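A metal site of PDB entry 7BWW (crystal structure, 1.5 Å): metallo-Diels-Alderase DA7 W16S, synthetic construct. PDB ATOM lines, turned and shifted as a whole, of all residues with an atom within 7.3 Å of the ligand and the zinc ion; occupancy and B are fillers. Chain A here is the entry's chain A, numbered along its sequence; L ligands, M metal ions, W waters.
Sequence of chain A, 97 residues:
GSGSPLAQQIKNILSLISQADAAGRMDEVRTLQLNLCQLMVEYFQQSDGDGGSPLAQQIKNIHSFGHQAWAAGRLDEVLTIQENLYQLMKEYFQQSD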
ATOM      1  N   GLN A  33       8.190  21.029  -9.151  1.00  0.00           N
ATOM      2  CA  GLN A  33       9.510  21.095  -8.526  1.00  0.00           C
ATOM      3  C   GLN A  33      10.606  21.311  -9.566  1.00  0.00           C
ATOM      4  O   GLN A  33      11.591  22.001  -9.278  1.00  0.00           O
ATOM      5  CB  GLN A  33       9.764  19.822  -7.717  1.00  0.00           C
ATOM      6  CG  GLN A  33       8.860  19.705  -6.497  1.00  0.00           C
ATOM      7  CD  GLN A  33       9.045  18.400  -5.751  1.00  0.00           C
ATOM      8  OE1 GLN A  33       9.161  17.330  -6.350  1.00  0.00           O
ATOM      9  NE2 GLN A  33       9.051  18.475  -4.426  1.00  0.00           N
ATOM     10  N   LEU A  34      10.448  20.759 -10.778  1.00  0.00           N
ATOM     11  CA  LEU A  34      11.388  21.041 -11.843  1.00  0.00           C
ATOM     12  C   LEU A  34      11.343  22.511 -12.210  1.00  0.00           C
ATOM     13  O   LEU A  34      12.370  23.144 -12.404  1.00  0.00           O
ATOM     14  CB  LEU A  34      11.079  20.171 -13.067  1.00  0.00           C
ATOM     15  CG  LEU A  34      11.294  18.670 -12.917  1.00  0.00           C
ATOM     16  CD1 LEU A  34      10.648  17.930 -14.085  1.00  0.00           C
ATOM     17  CD2 LEU A  34      12.791  18.370 -12.822  1.00  0.00           C
ATOM     18  N   LEU A  36      10.368  25.034 -10.242  1.00  0.00           N
ATOM     19  CA  LEU A  36      10.938  25.815  -9.141  1.00  0.00           C
ATOM     20  C   LEU A  36      12.469  25.781  -9.176  1.00  0.00           C
ATOM     21  O   LEU A  36      13.124  26.800  -8.920  1.00  0.00           O
ATOM     22  CB  LEU A  36      10.443  25.282  -7.793  1.00  0.00           C
ATOM     23  CG  LEU A  36      10.779  26.162  -6.594  1.00  0.00           C
ATOM     24  CD1 LEU A  36       9.968  27.444  -6.653  1.00  0.00           C
ATOM     25  CD2 LEU A  36      10.545  25.392  -5.283  1.00  0.00           C
ATOM     26  N   CYS A  37      13.040  24.604  -9.452  1.00  0.00           N
ATOM     27  CA  CYS A  37      14.484  24.486  -9.566  1.00  0.00           C
ATOM     28  C   CYS A  37      15.046  25.521 -10.535  1.00  0.00           C
ATOM     29  O   CYS A  37      15.942  26.296 -10.182  1.00  0.00           O
ATOM     30  CB  CYS A  37      14.832  23.065 -10.002  1.00  0.00           C
ATOM     31  SG  CYS A  37      16.541  22.870 -10.587  1.00  0.00           S
ATOM     32  N   GLN A  38      14.517  25.539 -11.763  1.00  0.00           N
ATOM     33  CA  GLN A  38      14.996  26.475 -12.780  1.00  0.00           C
ATOM     34  C   GLN A  38      14.812  27.917 -12.345  1.00  0.00           C
ATOM     35  O   GLN A  38      15.714  28.746 -12.519  1.00  0.00           O
ATOM     36  CB  GLN A  38      14.281  26.222 -14.115  1.00  0.00           C
ATOM     37  CG  GLN A  38      14.657  27.193 -15.249  1.00  0.00           C
ATOM     38  CD  GLN A  38      13.483  27.559 -16.142  1.00  0.00           C
ATOM     39  OE1 GLN A  38      12.316  27.480 -15.747  1.00  0.00           O
ATOM     40  NE2 GLN A  38      13.779  27.968 -17.379  1.00  0.00           N
ATOM     41  N   MET A  40      14.738  29.085  -9.336  1.00  0.00           N
ATOM     42  CA  MET A  40      15.721  29.417  -8.297  1.00  0.00           C
ATOM     43  C   MET A  40      17.097  29.701  -8.894  1.00  0.00           C
ATOM     44  O   MET A  40      17.800  30.612  -8.432  1.00  0.00           O
ATOM     45  CB  MET A  40      15.819  28.274  -7.283  1.00  0.00           C
ATOM     46  CG  MET A  40      14.613  28.156  -6.362  1.00  0.00           C
ATOM     47  SD  MET A  40      14.785  26.976  -4.997  1.00  0.00           S
ATOM     48  CE  MET A  40      14.764  25.361  -5.857  1.00  0.00           C
ATOM     49  N   VAL A  41      17.532  28.893  -9.858  1.00  0.00           N
ATOM     50  CA  VAL A  41      18.802  29.160 -10.533  1.00  0.00           C
ATOM     51  C   VAL A  41      18.789  30.571 -11.124  1.00  0.00           C
ATOM     52  O   VAL A  41      19.744  31.340 -10.975  1.00  0.00           O
ATOM     53  CB  VAL A  41      19.082  28.103 -11.617  1.00  0.00           C
ATOM     54  CG1 VAL A  41      20.338  28.469 -12.417  1.00  0.00           C
ATOM     55  CG2 VAL A  41      19.196  26.714 -10.978  1.00  0.00           C
ATOM     56  N   ILE A  62      22.286  25.609  -0.229  1.00  0.00           N
ATOM     57  CA  ILE A  62      21.485  24.416  -0.006  1.00  0.00           C
ATOM     58  C   ILE A  62      20.982  23.871  -1.340  1.00  0.00           C
ATOM     59  O   ILE A  62      20.992  22.657  -1.568  1.00  0.00           O
ATOM     60  CB  ILE A  62      20.331  24.735   0.951  1.00  0.00           C
ATOM     61  CG1 ILE A  62      20.909  25.008   2.347  1.00  0.00           C
ATOM     62  CG2 ILE A  62      19.341  23.592   1.005  1.00  0.00           C
ATOM     63  CD1 ILE A  62      19.898  25.728   3.260  1.00  0.00           C
ATOM     64  N   HIS A  63      20.588  24.751  -2.249  1.00  0.00           N
ATOM     65  CA  HIS A  63      20.189  24.282  -3.575  1.00  0.00           C
ATOM     66  C   HIS A  63      21.332  23.526  -4.260  1.00  0.00           C
ATOM     67  O   HIS A  63      21.115  22.453  -4.840  1.00  0.00           O
ATOM     68  CB  HIS A  63      19.761  25.488  -4.410  1.00  0.00           C
ATOM     69  CG  HIS A  63      19.079  25.136  -5.694  1.00  0.00           C
ATOM     70  ND1 HIS A  63      18.773  26.083  -6.648  1.00  0.00           N
ATOM     71  CD2 HIS A  63      18.612  23.957  -6.173  1.00  0.00           C
ATOM     72  CE1 HIS A  63      18.182  25.501  -7.672  1.00  0.00           C
ATOM     73  NE2 HIS A  63      18.058  24.217  -7.414  1.00  0.00           N
ATOM     74  N   SER A  64      22.547  24.043  -4.168  1.00  0.00           N
ATOM     75  CA  SER A  64      23.709  23.380  -4.754  1.00  0.00           C
ATOM     76  C   SER A  64      23.936  22.002  -4.151  1.00  0.00           C
ATOM     77  O   SER A  64      24.139  21.013  -4.872  1.00  0.00           O
ATOM     78  CB  SER A  64      24.945  24.256  -4.581  1.00  0.00           C
ATOM     79  OG  SER A  64      26.114  23.550  -4.983  1.00  0.00           O
ATOM     80  N   PHE A  65      23.907  21.907  -2.824  1.00  0.00           N
ATOM     81  CA  PHE A  65      24.073  20.597  -2.206  1.00  0.00           C
ATOM     82  C   PHE A  65      22.918  19.660  -2.528  1.00  0.00           C
ATOM     83  O   PHE A  65      23.111  18.438  -2.592  1.00  0.00           O
ATOM     84  CB  PHE A  65      24.266  20.751  -0.697  1.00  0.00           C
ATOM     85  CG  PHE A  65      25.525  21.445  -0.342  1.00  0.00           C
ATOM     86  CD1 PHE A  65      26.744  20.938  -0.748  1.00  0.00           C
ATOM     87  CD2 PHE A  65      25.513  22.652   0.352  1.00  0.00           C
ATOM     88  CE1 PHE A  65      27.940  21.589  -0.449  1.00  0.00           C
ATOM     89  CE2 PHE A  65      26.689  23.317   0.647  1.00  0.00           C
ATOM     90  CZ  PHE A  65      27.902  22.781   0.248  1.00  0.00           C
ATOM     91  N   GLY A  66      21.726  20.212  -2.766  1.00  0.00           N
ATOM     92  CA  GLY A  66      20.634  19.389  -3.224  1.00  0.00           C
ATOM     93  C   GLY A  66      20.914  18.743  -4.566  1.00  0.00           C
ATOM     94  O   GLY A  66      20.591  17.573  -4.791  1.00  0.00           O
ATOM     95  N   HIS A  67      21.498  19.500  -5.501  1.00  0.00           N
ATOM     96  CA  HIS A  67      21.874  18.901  -6.783  1.00  0.00           C
ATOM     97  C   HIS A  67      22.879  17.771  -6.583  1.00  0.00           C
ATOM     98  O   HIS A  67      22.779  16.723  -7.225  1.00  0.00           O
ATOM     99  CB  HIS A  67      22.437  19.952  -7.732  1.00  0.00           C
ATOM    100  CG  HIS A  67      21.378  20.735  -8.440  1.00  0.00           C
ATOM    101  ND1 HIS A  67      21.398  20.972  -9.796  1.00  0.00           N
ATOM    102  CD2 HIS A  67      20.252  21.325  -7.963  1.00  0.00           C
ATOM    103  CE1 HIS A  67      20.316  21.669 -10.130  1.00  0.00           C
ATOM    104  NE2 HIS A  67      19.607  21.882  -9.033  1.00  0.00           N
ATOM    105  N   GLN A  68      23.869  17.978  -5.712  1.00  0.00           N
ATOM    106  CA  GLN A  68      24.875  16.955  -5.501  1.00  0.00           C
ATOM    107  C   GLN A  68      24.257  15.688  -4.902  1.00  0.00           C
ATOM    108  O   GLN A  68      24.584  14.565  -5.330  1.00  0.00           O
ATOM    109  CB  GLN A  68      25.980  17.510  -4.611  1.00  0.00           C
ATOM    110  CG  GLN A  68      26.718  18.656  -5.270  1.00  0.00           C
ATOM    111  CD  GLN A  68      27.563  19.451  -4.285  1.00  0.00           C
ATOM    112  OE1 GLN A  68      28.299  18.884  -3.495  1.00  0.00           O
ATOM    113  NE2 GLN A  68      27.416  20.768  -4.311  1.00  0.00           N
ATOM    114  N   ALA A  69      23.323  15.856  -3.962  1.00  0.00           N
ATOM    115  CA  ALA A  69      22.665  14.687  -3.382  1.00  0.00           C
ATOM    116  C   ALA A  69      21.806  13.977  -4.416  1.00  0.00           C
ATOM    117  O   ALA A  69      21.801  12.742  -4.478  1.00  0.00           O
ATOM    118  CB  ALA A  69      21.788  15.121  -2.191  1.00  0.00           C
ATOM    119  N   TRP A  70      21.068  14.728  -5.222  1.00  0.00           N
ATOM    120  CA  TRP A  70      20.206  14.139  -6.238  1.00  0.00           C
ATOM    121  C   TRP A  70      21.025  13.350  -7.246  1.00  0.00           C
ATOM    122  O   TRP A  70      20.635  12.247  -7.649  1.00  0.00           O
ATOM    123  CB  TRP A  70      19.393  15.236  -6.916  1.00  0.00           C
ATOM    124  CG  TRP A  70      18.101  14.817  -7.466  1.00  0.00           C
ATOM    125  CD1 TRP A  70      16.878  14.957  -6.891  1.00  0.00           C
ATOM    126  CD2 TRP A  70      17.880  14.217  -8.756  1.00  0.00           C
ATOM    127  NE1 TRP A  70      15.907  14.462  -7.725  1.00  0.00           N
ATOM    128  CE2 TRP A  70      16.493  13.999  -8.877  1.00  0.00           C
ATOM    129  CE3 TRP A  70      18.724  13.833  -9.803  1.00  0.00           C
ATOM    130  CZ2 TRP A  70      15.927  13.410 -10.005  1.00  0.00           C
ATOM    131  CZ3 TRP A  70      18.153  13.247 -10.923  1.00  0.00           C
ATOM    132  CH2 TRP A  70      16.776  13.042 -11.020  1.00  0.00           C
ATOM    133  N   GLU A  77      18.940  12.185   1.791  1.00  0.00           N
ATOM    134  CA  GLU A  77      19.461  13.530   1.994  1.00  0.00           C
ATOM    135  C   GLU A  77      18.730  14.526   1.121  1.00  0.00           C
ATOM    136  O   GLU A  77      18.472  15.656   1.550  1.00  0.00           O
ATOM    137  CB  GLU A  77      20.975  13.525   1.749  1.00  0.00           C
ATOM    138  CG  GLU A  77      21.668  12.496   2.624  1.00  0.00           C
ATOM    139  CD  GLU A  77      23.168  12.691   2.828  1.00  0.00           C
ATOM    140  OE1 GLU A  77      23.813  11.728   3.272  1.00  0.00           O
ATOM    141  OE2 GLU A  77      23.717  13.779   2.572  1.00  0.00           O
ATOM    142  N   VAL A  78      18.312  14.130  -0.084  1.00  0.00           N
ATOM    143  CA  VAL A  78      17.482  14.996  -0.920  1.00  0.00           C
ATOM    144  C   VAL A  78      16.246  15.462  -0.165  1.00  0.00           C
ATOM    145  O   VAL A  78      15.876  16.639  -0.219  1.00  0.00           O
ATOM    146  CB  VAL A  78      17.092  14.279  -2.228  1.00  0.00           C
ATOM    147  CG1 VAL A  78      15.954  15.029  -2.921  1.00  0.00           C
ATOM    148  CG2 VAL A  78      18.308  14.131  -3.114  1.00  0.00           C
ATOM    149  N   LEU A  79      15.586  14.542   0.544  1.00  0.00           N
ATOM    150  CA  LEU A  79      14.299  14.886   1.134  1.00  0.00           C
ATOM    151  C   LEU A  79      14.449  15.886   2.286  1.00  0.00           C
ATOM    152  O   LEU A  79      13.599  16.774   2.433  1.00  0.00           O
ATOM    153  CB  LEU A  79      13.587  13.632   1.617  1.00  0.00           C
ATOM    154  CG  LEU A  79      13.166  12.726   0.463  1.00  0.00           C
ATOM    155  CD1 LEU A  79      12.658  11.415   1.006  1.00  0.00           C
ATOM    156  CD2 LEU A  79      12.089  13.393  -0.406  1.00  0.00           C
ATOM    157  N   THR A  80      15.485  15.742   3.122  1.00  0.00           N
ATOM    158  CA  THR A  80      15.603  16.711   4.206  1.00  0.00           C
ATOM    159  C   THR A  80      16.274  17.998   3.738  1.00  0.00           C
ATOM    160  O   THR A  80      15.988  19.068   4.290  1.00  0.00           O
ATOM    161  CB  THR A  80      16.321  16.107   5.404  1.00  0.00           C
ATOM    162  OG1 THR A  80      17.622  15.645   5.040  1.00  0.00           O
ATOM    163  CG2 THR A  80      15.490  14.944   6.004  1.00  0.00           C
ATOM    164  N   ILE A  81      17.108  17.937   2.682  1.00  0.00           N
ATOM    165  CA  ILE A  81      17.549  19.167   2.045  1.00  0.00           C
ATOM    166  C   ILE A  81      16.342  19.920   1.492  1.00  0.00           C
ATOM    167  O   ILE A  81      16.230  21.150   1.658  1.00  0.00           O
ATOM    168  CB  ILE A  81      18.570  18.859   0.938  1.00  0.00           C
ATOM    169  CG1 ILE A  81      19.918  18.520   1.549  1.00  0.00           C
ATOM    170  CG2 ILE A  81      18.724  20.074  -0.006  1.00  0.00           C
ATOM    171  CD1 ILE A  81      20.937  17.900   0.534  1.00  0.00           C
ATOM    172  N   GLN A  82      15.415  19.208   0.838  1.00  0.00           N
ATOM    173  CA  GLN A  82      14.214  19.850   0.303  1.00  0.00           C
ATOM    174  C   GLN A  82      13.415  20.531   1.406  1.00  0.00           C
ATOM    175  O   GLN A  82      12.970  21.675   1.238  1.00  0.00           O
ATOM    176  CB  GLN A  82      13.354  18.816  -0.420  1.00  0.00           C
ATOM    177  CG  GLN A  82      12.080  19.418  -1.054  1.00  0.00           C
ATOM    178  CD  GLN A  82      11.029  18.364  -1.387  1.00  0.00           C
ATOM    179  OE1 GLN A  82       9.831  18.626  -1.304  1.00  0.00           O
ATOM    180  NE2 GLN A  82      11.473  17.183  -1.743  1.00  0.00           N
ATOM    181  N   GLU A  83      13.237  19.858   2.548  1.00  0.00           N
ATOM    182  CA  GLU A  83      12.493  20.465   3.648  1.00  0.00           C
ATOM    183  C   GLU A  83      13.133  21.773   4.060  1.00  0.00           C
ATOM    184  O   GLU A  83      12.446  22.793   4.240  1.00  0.00           O
ATOM    185  CB  GLU A  83      12.417  19.513   4.845  1.00  0.00           C
ATOM    186  CG  GLU A  83      11.534  18.296   4.625  1.00  0.00           C
ATOM    187  CD  GLU A  83      11.718  17.223   5.697  1.00  0.00           C
ATOM    188  OE1 GLU A  83      12.384  17.508   6.720  1.00  0.00           O
ATOM    189  OE2 GLU A  83      11.204  16.099   5.507  1.00  0.00           O
ATOM    190  N   LEU A  85      15.368  23.698   2.286  1.00  0.00           N
ATOM    191  CA  LEU A  85      15.356  24.656   1.181  1.00  0.00           C
ATOM    192  C   LEU A  85      13.992  25.289   1.010  1.00  0.00           C
ATOM    193  O   LEU A  85      13.880  26.512   0.833  1.00  0.00           O
ATOM    194  CB  LEU A  85      15.764  23.924  -0.110  1.00  0.00           C
ATOM    195  CG  LEU A  85      15.776  24.765  -1.389  1.00  0.00           C
ATOM    196  CD1 LEU A  85      16.745  25.940  -1.322  1.00  0.00           C
ATOM    197  CD2 LEU A  85      16.131  23.860  -2.567  1.00  0.00           C
ATOM    198  N   TYR A  86      12.931  24.478   1.043  1.00  0.00           N
ATOM    199  CA  TYR A  86      11.617  25.026   0.774  1.00  0.00           C
ATOM    200  C   TYR A  86      11.145  25.907   1.931  1.00  0.00           C
ATOM    201  O   TYR A  86      10.480  26.910   1.689  1.00  0.00           O
ATOM    202  CB  TYR A  86      10.603  23.910   0.471  1.00  0.00           C
ATOM    203  CG  TYR A  86      10.764  23.269  -0.904  1.00  0.00           C
ATOM    204  CD1 TYR A  86      11.841  23.566  -1.743  1.00  0.00           C
ATOM    205  CD2 TYR A  86       9.819  22.353  -1.367  1.00  0.00           C
ATOM    206  CE1 TYR A  86      11.967  22.946  -3.013  1.00  0.00           C
ATOM    207  CE2 TYR A  86       9.921  21.764  -2.613  1.00  0.00           C
ATOM    208  CZ  TYR A  86      11.000  22.054  -3.437  1.00  0.00           C
ATOM    209  OH  TYR A  86      11.078  21.427  -4.684  1.00  0.00           O
HETATM  210  C1  LIG L   1      16.304  21.318  -6.558  1.00  0.00           C
HETATM  211  O1  LIG L   1      15.381  22.111  -6.837  1.00  0.00           O
HETATM  212  O2  LIG L   1      17.272  21.203  -7.331  1.00  0.00           O
HETATM  213  C2  LIG L   1      16.273  20.480  -5.327  1.00  0.00           C
HETATM  214  C3  LIG L   1      15.289  20.703  -4.373  1.00  0.00           C
HETATM  215  C4  LIG L   1      15.259  19.920  -3.219  1.00  0.00           C
HETATM  216  C5  LIG L   1      16.201  18.913  -3.037  1.00  0.00           C
HETATM  217  C6  LIG L   1      17.191  18.702  -3.979  1.00  0.00           C
HETATM  218  C7  LIG L   1      17.215  19.473  -5.144  1.00  0.00           C
HETATM  219 ZN    ZN M   1      17.702  22.605  -8.675  1.00  0.00          ZN
HETATM  220  O   HOH W   1      12.691  22.254  -6.622  1.00  0.00           O
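OE1 of Gln 82 sits at hydrogen-bond distance from NE2 of Gln 33 (3.2 Å).
Water W1 lies within hydrogen-bond range of OH of Tyr 86 (2.7 Å), O1 of the ligand (2.7 Å) and O of Gln 33 (2.9 Å).
Of the 25 residues printed, 3 come within 4 Å of the zinc ion. The nearest printed residue that does not touch the zinc ion is Met 40 (4.9 Å).
Residues that only touch the ligand: Met 40 (3.5 Å), Gly 66 (3.6 Å), Val 78 (3.6 Å), Gln 82 (3.6 Å) and Leu 85 (3.7 Å). Hydrophobic or aromatic side chains within 4 Å of the ligand: Met 40, His 63, His 67, Val 78 and Leu 85. Within 4 Å of the ligand: Cys 37, Met 40, His 63, Gly 66, His 67, Val 78, Gln 82 and Leu 85.
The zinc ion is bound by O2 of the ligand, at 2.0 Å. The zinc ion is bound by a ring nitrogen (NE2) of His 67 (2.1 Å). NE2 of His 63 binds the zinc ion, 2.1 Å away. The side-chain sulfur (SG) of Cys 37 binds the zinc ion, at 2.3 Å. The zinc ion has four donor atoms within binding distance.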
